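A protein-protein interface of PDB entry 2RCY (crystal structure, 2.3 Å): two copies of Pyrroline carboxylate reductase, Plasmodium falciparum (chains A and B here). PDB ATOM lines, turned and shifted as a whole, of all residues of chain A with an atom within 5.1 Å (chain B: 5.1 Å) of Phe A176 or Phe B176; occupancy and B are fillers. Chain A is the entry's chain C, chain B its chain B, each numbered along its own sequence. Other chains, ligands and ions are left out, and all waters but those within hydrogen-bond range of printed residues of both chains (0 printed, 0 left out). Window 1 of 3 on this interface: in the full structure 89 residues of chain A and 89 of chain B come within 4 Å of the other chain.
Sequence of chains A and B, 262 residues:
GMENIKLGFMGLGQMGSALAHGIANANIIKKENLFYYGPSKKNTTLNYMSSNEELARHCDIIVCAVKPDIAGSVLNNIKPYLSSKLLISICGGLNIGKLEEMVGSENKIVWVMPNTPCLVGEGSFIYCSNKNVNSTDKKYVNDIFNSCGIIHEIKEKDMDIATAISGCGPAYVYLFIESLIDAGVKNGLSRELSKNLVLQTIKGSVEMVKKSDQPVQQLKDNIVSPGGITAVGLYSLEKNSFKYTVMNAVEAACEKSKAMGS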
ATOM      1  N   ALA A 171     -12.092  -8.395  -7.084  1.00  0.00           N
ATOM      2  CA  ALA A 171     -11.015  -9.349  -6.814  1.00  0.00           C
ATOM      3  C   ALA A 171      -9.985  -9.412  -7.941  1.00  0.00           C
ATOM      4  O   ALA A 171      -8.787  -9.521  -7.678  1.00  0.00           O
ATOM      5  CB  ALA A 171     -11.582 -10.728  -6.548  1.00  0.00           C
ATOM      6  N   TYR A 172     -10.454  -9.347  -9.188  1.00  0.00           N
ATOM      7  CA  TYR A 172      -9.563  -9.350 -10.345  1.00  0.00           C
ATOM      8  C   TYR A 172      -8.773  -8.045 -10.386  1.00  0.00           C
ATOM      9  O   TYR A 172      -7.571  -8.047 -10.650  1.00  0.00           O
ATOM     10  CB  TYR A 172     -10.327  -9.527 -11.667  1.00  0.00           C
ATOM     11  CG  TYR A 172     -11.408 -10.596 -11.698  1.00  0.00           C
ATOM     12  CD1 TYR A 172     -12.566 -10.405 -12.451  1.00  0.00           C
ATOM     13  CD2 TYR A 172     -11.274 -11.794 -10.993  1.00  0.00           C
ATOM     14  CE1 TYR A 172     -13.562 -11.371 -12.500  1.00  0.00           C
ATOM     15  CE2 TYR A 172     -12.267 -12.767 -11.033  1.00  0.00           C
ATOM     16  CZ  TYR A 172     -13.407 -12.548 -11.789  1.00  0.00           C
ATOM     17  OH  TYR A 172     -14.399 -13.503 -11.836  1.00  0.00           O
ATOM     18  N   VAL A 173      -9.467  -6.939 -10.117  1.00  0.00           N
ATOM     19  CA  VAL A 173      -8.857  -5.613 -10.106  1.00  0.00           C
ATOM     20  C   VAL A 173      -7.843  -5.497  -8.967  1.00  0.00           C
ATOM     21  O   VAL A 173      -6.747  -4.977  -9.171  1.00  0.00           O
ATOM     22  CB  VAL A 173      -9.915  -4.480 -10.014  1.00  0.00           C
ATOM     23  CG1 VAL A 173      -9.264  -3.116 -10.231  1.00  0.00           C
ATOM     24  CG2 VAL A 173     -11.023  -4.692 -11.041  1.00  0.00           C
ATOM     25  N   TYR A 174      -8.198  -5.998  -7.784  1.00  0.00           N
ATOM     26  CA  TYR A 174      -7.274  -6.023  -6.649  1.00  0.00           C
ATOM     27  C   TYR A 174      -5.999  -6.796  -6.987  1.00  0.00           C
ATOM     28  O   TYR A 174      -4.897  -6.319  -6.720  1.00  0.00           O
ATOM     29  CB  TYR A 174      -7.928  -6.609  -5.391  1.00  0.00           C
ATOM     30  CG  TYR A 174      -9.033  -5.767  -4.778  1.00  0.00           C
ATOM     31  CD1 TYR A 174      -8.897  -4.385  -4.628  1.00  0.00           C
ATOM     32  CD2 TYR A 174     -10.207  -6.363  -4.319  1.00  0.00           C
ATOM     33  CE1 TYR A 174      -9.914  -3.619  -4.058  1.00  0.00           C
ATOM     34  CE2 TYR A 174     -11.225  -5.609  -3.751  1.00  0.00           C
ATOM     35  CZ  TYR A 174     -11.074  -4.242  -3.621  1.00  0.00           C
ATOM     36  OH  TYR A 174     -12.088  -3.505  -3.053  1.00  0.00           O
ATOM     37  N   LEU A 175      -6.159  -7.979  -7.581  1.00  0.00           N
ATOM     38  CA  LEU A 175      -5.029  -8.814  -7.999  1.00  0.00           C
ATOM     39  C   LEU A 175      -4.199  -8.109  -9.074  1.00  0.00           C
ATOM     40  O   LEU A 175      -2.970  -8.183  -9.062  1.00  0.00           O
ATOM     41  CB  LEU A 175      -5.522 -10.170  -8.517  1.00  0.00           C
ATOM     42  CG  LEU A 175      -4.702 -11.443  -8.250  1.00  0.00           C
ATOM     43  CD1 LEU A 175      -5.450 -12.650  -8.776  1.00  0.00           C
ATOM     44  CD2 LEU A 175      -3.303 -11.416  -8.845  1.00  0.00           C
ATOM     45  N   PHE A 176      -4.885  -7.432  -9.994  1.00  0.00           N
ATOM     46  CA  PHE A 176      -4.248  -6.632 -11.037  1.00  0.00           C
ATOM     47  C   PHE A 176      -3.396  -5.518 -10.423  1.00  0.00           C
ATOM     48  O   PHE A 176      -2.230  -5.352 -10.790  1.00  0.00           O
ATOM     49  CB  PHE A 176      -5.317  -6.059 -11.980  1.00  0.00           C
ATOM     50  CG  PHE A 176      -4.764  -5.328 -13.175  1.00  0.00           C
ATOM     51  CD1 PHE A 176      -3.845  -5.938 -14.026  1.00  0.00           C
ATOM     52  CD2 PHE A 176      -5.189  -4.038 -13.466  1.00  0.00           C
ATOM     53  CE1 PHE A 176      -3.342  -5.264 -15.135  1.00  0.00           C
ATOM     54  CE2 PHE A 176      -4.694  -3.357 -14.573  1.00  0.00           C
ATOM     55  CZ  PHE A 176      -3.769  -3.972 -15.410  1.00  0.00           C
ATOM     56  N   ILE A 177      -3.986  -4.781  -9.481  1.00  0.00           N
ATOM     57  CA  ILE A 177      -3.299  -3.723  -8.736  1.00  0.00           C
ATOM     58  C   ILE A 177      -2.124  -4.296  -7.935  1.00  0.00           C
ATOM     59  O   ILE A 177      -1.021  -3.749  -7.961  1.00  0.00           O
ATOM     60  CB  ILE A 177      -4.285  -2.961  -7.799  1.00  0.00           C
ATOM     61  CG1 ILE A 177      -5.291  -2.152  -8.627  1.00  0.00           C
ATOM     62  CG2 ILE A 177      -3.536  -2.044  -6.828  1.00  0.00           C
ATOM     63  CD1 ILE A 177      -6.515  -1.670  -7.852  1.00  0.00           C
ATOM     64  N   GLU A 178      -2.375  -5.406  -7.245  1.00  0.00           N
ATOM     65  CA  GLU A 178      -1.370  -6.112  -6.448  1.00  0.00           C
ATOM     66  C   GLU A 178      -0.162  -6.536  -7.287  1.00  0.00           C
ATOM     67  O   GLU A 178       0.980  -6.434  -6.833  1.00  0.00           O
ATOM     68  CB  GLU A 178      -2.017  -7.334  -5.779  1.00  0.00           C
ATOM     69  CG  GLU A 178      -1.083  -8.256  -5.005  1.00  0.00           C
ATOM     70  CD  GLU A 178      -1.758  -9.559  -4.601  1.00  0.00           C
ATOM     71  OE1 GLU A 178      -3.004  -9.623  -4.620  1.00  0.00           O
ATOM     72  OE2 GLU A 178      -1.044 -10.523  -4.261  1.00  0.00           O
ATOM     73  N   SER A 179      -0.428  -6.998  -8.508  1.00  0.00           N
ATOM     74  CA  SER A 179       0.614  -7.489  -9.411  1.00  0.00           C
ATOM     75  C   SER A 179       1.464  -6.358  -9.984  1.00  0.00           C
ATOM     76  O   SER A 179       2.671  -6.519 -10.180  1.00  0.00           O
ATOM     77  CB  SER A 179      -0.004  -8.310 -10.548  1.00  0.00           C
ATOM     78  OG  SER A 179      -0.831  -9.345 -10.044  1.00  0.00           O
ATOM     79  N   LEU A 180       0.827  -5.218 -10.251  1.00  0.00           N
ATOM     80  CA  LEU A 180       1.516  -4.044 -10.789  1.00  0.00           C
ATOM     81  C   LEU A 180       2.460  -3.428  -9.757  1.00  0.00           C
ATOM     82  O   LEU A 180       3.557  -2.978 -10.102  1.00  0.00           O
ATOM     83  CB  LEU A 180       0.511  -3.005 -11.303  1.00  0.00           C
ATOM     84  CG  LEU A 180      -0.278  -3.292 -12.591  1.00  0.00           C
ATOM     85  CD1 LEU A 180      -1.489  -2.381 -12.691  1.00  0.00           C
ATOM     86  CD2 LEU A 180       0.588  -3.156 -13.840  1.00  0.00           C
ATOM     87  N   ILE A 202      -4.548   3.780 -13.384  1.00  0.00           N
ATOM     88  CA  ILE A 202      -5.836   3.127 -13.601  1.00  0.00           C
ATOM     89  C   ILE A 202      -6.984   4.139 -13.588  1.00  0.00           C
ATOM     90  O   ILE A 202      -7.860   4.094 -14.453  1.00  0.00           O
ATOM     91  CB  ILE A 202      -6.093   2.003 -12.568  1.00  0.00           C
ATOM     92  CG1 ILE A 202      -4.979   0.954 -12.630  1.00  0.00           C
ATOM     93  CG2 ILE A 202      -7.440   1.346 -12.824  1.00  0.00           C
ATOM     94  CD1 ILE A 202      -4.997  -0.046 -11.495  1.00  0.00           C
ATOM     95  N   PHE A 242      -2.707 -12.840 -21.719  1.00  0.00           N
ATOM     96  CA  PHE A 242      -3.349 -11.958 -20.740  1.00  0.00           C
ATOM     97  C   PHE A 242      -4.856 -11.816 -20.957  1.00  0.00           C
ATOM     98  O   PHE A 242      -5.634 -11.911 -20.005  1.00  0.00           O
ATOM     99  CB  PHE A 242      -2.675 -10.582 -20.754  1.00  0.00           C
ATOM    100  CG  PHE A 242      -3.293  -9.584 -19.817  1.00  0.00           C
ATOM    101  CD1 PHE A 242      -3.002  -9.612 -18.457  1.00  0.00           C
ATOM    102  CD2 PHE A 242      -4.151  -8.602 -20.297  1.00  0.00           C
ATOM    103  CE1 PHE A 242      -3.568  -8.682 -17.590  1.00  0.00           C
ATOM    104  CE2 PHE A 242      -4.721  -7.669 -19.435  1.00  0.00           C
ATOM    105  CZ  PHE A 242      -4.428  -7.711 -18.080  1.00  0.00           C
ATOM    106  N   VAL A 246      -7.929 -13.298 -18.371  1.00  0.00           N
ATOM    107  CA  VAL A 246      -8.977 -12.458 -17.797  1.00  0.00           C
ATOM    108  C   VAL A 246     -10.361 -12.986 -18.197  1.00  0.00           C
ATOM    109  O   VAL A 246     -11.253 -13.110 -17.354  1.00  0.00           O
ATOM    110  CB  VAL A 246      -8.801 -10.968 -18.214  1.00  0.00           C
ATOM    111  CG1 VAL A 246      -9.942 -10.110 -17.693  1.00  0.00           C
ATOM    112  CG2 VAL A 246      -7.469 -10.421 -17.713  1.00  0.00           C
ATOM    113  N   ALA B 171      -2.059   1.329 -21.277  1.00  0.00           N
ATOM    114  CA  ALA B 171      -2.255   0.277 -22.276  1.00  0.00           C
ATOM    115  C   ALA B 171      -2.598  -1.073 -21.651  1.00  0.00           C
ATOM    116  O   ALA B 171      -3.379  -1.837 -22.221  1.00  0.00           O
ATOM    117  CB  ALA B 171      -1.036   0.154 -23.166  1.00  0.00           C
ATOM    118  N   TYR B 172      -2.009  -1.366 -20.491  1.00  0.00           N
ATOM    119  CA  TYR B 172      -2.319  -2.597 -19.763  1.00  0.00           C
ATOM    120  C   TYR B 172      -3.734  -2.524 -19.201  1.00  0.00           C
ATOM    121  O   TYR B 172      -4.448  -3.527 -19.176  1.00  0.00           O
ATOM    122  CB  TYR B 172      -1.341  -2.854 -18.607  1.00  0.00           C
ATOM    123  CG  TYR B 172       0.130  -2.621 -18.880  1.00  0.00           C
ATOM    124  CD1 TYR B 172       0.944  -2.061 -17.900  1.00  0.00           C
ATOM    125  CD2 TYR B 172       0.715  -2.970 -20.100  1.00  0.00           C
ATOM    126  CE1 TYR B 172       2.296  -1.842 -18.123  1.00  0.00           C
ATOM    127  CE2 TYR B 172       2.072  -2.753 -20.334  1.00  0.00           C
ATOM    128  CZ  TYR B 172       2.855  -2.189 -19.338  1.00  0.00           C
ATOM    129  OH  TYR B 172       4.195  -1.964 -19.550  1.00  0.00           O
ATOM    130  N   VAL B 173      -4.121  -1.333 -18.745  1.00  0.00           N
ATOM    131  CA  VAL B 173      -5.438  -1.111 -18.156  1.00  0.00           C
ATOM    132  C   VAL B 173      -6.521  -1.134 -19.236  1.00  0.00           C
ATOM    133  O   VAL B 173      -7.587  -1.710 -19.025  1.00  0.00           O
ATOM    134  CB  VAL B 173      -5.497   0.207 -17.333  1.00  0.00           C
ATOM    135  CG1 VAL B 173      -6.854   0.362 -16.652  1.00  0.00           C
ATOM    136  CG2 VAL B 173      -4.390   0.239 -16.286  1.00  0.00           C
ATOM    137  N   TYR B 174      -6.238  -0.522 -20.388  1.00  0.00           N
ATOM    138  CA  TYR B 174      -7.159  -0.551 -21.527  1.00  0.00           C
ATOM    139  C   TYR B 174      -7.404  -1.980 -22.003  1.00  0.00           C
ATOM    140  O   TYR B 174      -8.534  -2.340 -22.332  1.00  0.00           O
ATOM    141  CB  TYR B 174      -6.638   0.283 -22.706  1.00  0.00           C
ATOM    142  CG  TYR B 174      -6.583   1.782 -22.491  1.00  0.00           C
ATOM    143  CD1 TYR B 174      -7.598   2.459 -21.813  1.00  0.00           C
ATOM    144  CD2 TYR B 174      -5.524   2.530 -23.006  1.00  0.00           C
ATOM    145  CE1 TYR B 174      -7.540   3.840 -21.630  1.00  0.00           C
ATOM    146  CE2 TYR B 174      -5.459   3.902 -22.832  1.00  0.00           C
ATOM    147  CZ  TYR B 174      -6.466   4.551 -22.148  1.00  0.00           C
ATOM    148  OH  TYR B 174      -6.390   5.913 -21.983  1.00  0.00           O
ATOM    149  N   LEU B 175      -6.340  -2.781 -22.044  1.00  0.00           N
ATOM    150  CA  LEU B 175      -6.436  -4.185 -22.437  1.00  0.00           C
ATOM    151  C   LEU B 175      -7.201  -4.992 -21.389  1.00  0.00           C
ATOM    152  O   LEU B 175      -7.960  -5.902 -21.729  1.00  0.00           O
ATOM    153  CB  LEU B 175      -5.041  -4.783 -22.679  1.00  0.00           C
ATOM    154  CG  LEU B 175      -4.939  -6.224 -23.205  1.00  0.00           C
ATOM    155  CD1 LEU B 175      -5.650  -6.403 -24.543  1.00  0.00           C
ATOM    156  CD2 LEU B 175      -3.487  -6.657 -23.319  1.00  0.00           C
ATOM    157  N   PHE B 176      -6.991  -4.642 -20.120  1.00  0.00           N
ATOM    158  CA  PHE B 176      -7.691  -5.253 -18.992  1.00  0.00           C
ATOM    159  C   PHE B 176      -9.190  -4.971 -19.090  1.00  0.00           C
ATOM    160  O   PHE B 176     -10.009  -5.879 -18.928  1.00  0.00           O
ATOM    161  CB  PHE B 176      -7.113  -4.718 -17.675  1.00  0.00           C
ATOM    162  CG  PHE B 176      -7.659  -5.386 -16.443  1.00  0.00           C
ATOM    163  CD1 PHE B 176      -7.384  -6.723 -16.174  1.00  0.00           C
ATOM    164  CD2 PHE B 176      -8.423  -4.663 -15.533  1.00  0.00           C
ATOM    165  CE1 PHE B 176      -7.882  -7.337 -15.027  1.00  0.00           C
ATOM    166  CE2 PHE B 176      -8.922  -5.268 -14.382  1.00  0.00           C
ATOM    167  CZ  PHE B 176      -8.652  -6.609 -14.130  1.00  0.00           C
ATOM    168  N   ILE B 177      -9.529  -3.712 -19.370  1.00  0.00           N
ATOM    169  CA  ILE B 177     -10.914  -3.279 -19.580  1.00  0.00           C
ATOM    170  C   ILE B 177     -11.509  -3.994 -20.795  1.00  0.00           C
ATOM    171  O   ILE B 177     -12.605  -4.551 -20.720  1.00  0.00           O
ATOM    172  CB  ILE B 177     -11.005  -1.735 -19.749  1.00  0.00           C
ATOM    173  CG1 ILE B 177     -10.610  -1.029 -18.447  1.00  0.00           C
ATOM    174  CG2 ILE B 177     -12.408  -1.305 -20.173  1.00  0.00           C
ATOM    175  CD1 ILE B 177     -10.245   0.438 -18.606  1.00  0.00           C
ATOM    176  N   GLU B 178     -10.764  -3.981 -21.898  1.00  0.00           N
ATOM    177  CA  GLU B 178     -11.136  -4.655 -23.143  1.00  0.00           C
ATOM    178  C   GLU B 178     -11.484  -6.134 -22.938  1.00  0.00           C
ATOM    179  O   GLU B 178     -12.492  -6.619 -23.457  1.00  0.00           O
ATOM    180  CB  GLU B 178      -9.989  -4.512 -24.149  1.00  0.00           C
ATOM    181  CG  GLU B 178     -10.172  -5.216 -25.485  1.00  0.00           C
ATOM    182  CD  GLU B 178      -8.942  -5.096 -26.369  1.00  0.00           C
ATOM    183  OE1 GLU B 178      -8.151  -4.148 -26.169  1.00  0.00           O
ATOM    184  OE2 GLU B 178      -8.765  -5.943 -27.269  1.00  0.00           O
ATOM    185  N   SER B 179     -10.645  -6.833 -22.174  1.00  0.00           N
ATOM    186  CA  SER B 179     -10.797  -8.266 -21.930  1.00  0.00           C
ATOM    187  C   SER B 179     -12.012  -8.577 -21.054  1.00  0.00           C
ATOM    188  O   SER B 179     -12.661  -9.611 -21.229  1.00  0.00           O
ATOM    189  CB  SER B 179      -9.526  -8.834 -21.289  1.00  0.00           C
ATOM    190  OG  SER B 179      -8.378  -8.528 -22.063  1.00  0.00           O
ATOM    191  N   LEU B 180     -12.308  -7.679 -20.117  1.00  0.00           N
ATOM    192  CA  LEU B 180     -13.473  -7.812 -19.246  1.00  0.00           C
ATOM    193  C   LEU B 180     -14.775  -7.524 -19.993  1.00  0.00           C
ATOM    194  O   LEU B 180     -15.812  -8.126 -19.695  1.00  0.00           O
ATOM    195  CB  LEU B 180     -13.346  -6.892 -18.027  1.00  0.00           C
ATOM    196  CG  LEU B 180     -12.342  -7.229 -16.918  1.00  0.00           C
ATOM    197  CD1 LEU B 180     -12.064  -6.000 -16.077  1.00  0.00           C
ATOM    198  CD2 LEU B 180     -12.822  -8.379 -16.038  1.00  0.00           C
ATOM    199  N   ILE B 202     -14.075  -1.198 -11.606  1.00  0.00           N
ATOM    200  CA  ILE B 202     -12.691  -0.747 -11.462  1.00  0.00           C
ATOM    201  C   ILE B 202     -12.627   0.558 -10.665  1.00  0.00           C
ATOM    202  O   ILE B 202     -11.794   0.698  -9.766  1.00  0.00           O
ATOM    203  CB  ILE B 202     -11.976  -0.586 -12.828  1.00  0.00           C
ATOM    204  CG1 ILE B 202     -11.925  -1.924 -13.572  1.00  0.00           C
ATOM    205  CG2 ILE B 202     -10.560  -0.063 -12.629  1.00  0.00           C
ATOM    206  CD1 ILE B 202     -11.513  -1.808 -15.031  1.00  0.00           C
ATOM    207  N   PHE B 242      -1.706 -15.203 -13.748  1.00  0.00           N
ATOM    208  CA  PHE B 242      -2.113 -13.811 -13.965  1.00  0.00           C
ATOM    209  C   PHE B 242      -1.112 -12.798 -13.400  1.00  0.00           C
ATOM    210  O   PHE B 242      -0.759 -11.832 -14.079  1.00  0.00           O
ATOM    211  CB  PHE B 242      -3.515 -13.556 -13.397  1.00  0.00           C
ATOM    212  CG  PHE B 242      -3.996 -12.139 -13.569  1.00  0.00           C
ATOM    213  CD1 PHE B 242      -4.486 -11.697 -14.795  1.00  0.00           C
ATOM    214  CD2 PHE B 242      -3.963 -11.247 -12.503  1.00  0.00           C
ATOM    215  CE1 PHE B 242      -4.933 -10.387 -14.956  1.00  0.00           C
ATOM    216  CE2 PHE B 242      -4.405  -9.936 -12.653  1.00  0.00           C
ATOM    217  CZ  PHE B 242      -4.891  -9.504 -13.882  1.00  0.00           C
ATOM    218  N   VAL B 246       1.317 -10.105 -15.650  1.00  0.00           N
ATOM    219  CA  VAL B 246       1.303  -8.661 -15.436  1.00  0.00           C
ATOM    220  C   VAL B 246       2.704  -8.154 -15.062  1.00  0.00           C
ATOM    221  O   VAL B 246       3.185  -7.173 -15.637  1.00  0.00           O
ATOM    222  CB  VAL B 246       0.254  -8.258 -14.360  1.00  0.00           C
ATOM    223  CG1 VAL B 246       0.273  -6.763 -14.112  1.00  0.00           C
ATOM    224  CG2 VAL B 246      -1.141  -8.693 -14.784  1.00  0.00           C
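Printed residues of chain B that touch a printed residue of chain A: Tyr B172, Val B173, Leu B175, Phe B176, Ser B179, Leu B180, Ile B202, Phe B242 and Val B246. Hydrophobic or aromatic side chains of chain A that line the printed part of chain B: Val A173, Leu A175, Phe A176, Leu A180, Ile A202, Phe A242 and Val A246. Among the printed residues, no Asp or Glu carboxylate lies within 4 Å of a Lys or Arg side-chain nitrogen of the other chain.
Among the printed residues, pairs that only touch across the chains: Tyr A172 with Phe B176 (3.9 Å), Val A173 with Phe B176 (3.99 Å), Val A173 with Ile B202 (3.9 Å), Leu A175 with Phe B242 (3.7 Å), Phe A176 with Tyr B172 (3.9 Å), Phe A176 with Val B173 (3.99 Å), Phe A176 with Phe B176 (3.9 Å), Phe A176 with Phe B242 (3.7 Å), Phe A176 with Val B246 (3.9 Å), Ser A179 with Val B246 (3.8 Å), Leu A180 with Val B246 (3.6 Å), Ile A202 with Val B173 (3.8 Å), Ile A202 with Ile B202 (3.4 Å), Phe A242 with Leu B175 (3.7 Å), Phe A242 with Phe B176 (3.7 Å), Phe A242 with Phe B242 (3.4 Å), Phe A242 with Val B246 (3.7 Å), Val A246 with Ser B179 (3.8 Å), Val A246 with Leu B180 (3.7 Å) and Val A246 with Phe B242 (3.7 Å).
OG of Ser B179 lies within hydrogen-bond range of O of Leu B175 (2.7 Å). The side-chain hydroxyl (OG) of Ser A179 lies within hydrogen-bond range of the backbone carbonyl oxygen (O) of Leu A175 (2.6 Å).
Of the printed residues of chain B, Phe A176 touches Tyr B172, Val B173, Phe B176, Phe B242 and Val B246. Printed residues of chain A within 4 Å of Phe B176: Tyr A172, Val A173, Phe A176 and Phe A242. Of the printed residues of chain B, Ser A179 touches Val B246. Of the printed residues of chain A, Leu B175 touches Phe A242 (3.7 Å). Of the printed residues of chain B, Phe A242 touches Leu B175 (3.7 Å), Phe B176 (3.7 Å), Phe B242 (3.4 Å) and Val B246 (3.7 Å). Of the printed residues of chain A, Val B246 touches Phe A176, Ser A179, Leu A180 and Phe A242. Glu B178 touches none of the printed residues of chain A. The nearest printed residue of chain A that does not touch Phe B176 is Val A246 (4.01 Å). The nearest printed residue of chain B that does not touch Ile A202 is Ile B177 (6.0 Å).
Val A173 touches Ile B202, and with the chains exchanged Ile A202 touches Val B173. Leu A175 touches Phe B242, and with the chains exchanged Phe A242 touches Leu B175. Phe B176 touches its own counterpart, Phe A176. Leu A180 touches Val B246, and with the chains exchanged Val A246 touches Leu B180. Of the 20 pairs that touch across the chains among the printed residues, 19 have their exchanged pair printed and touching as well.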
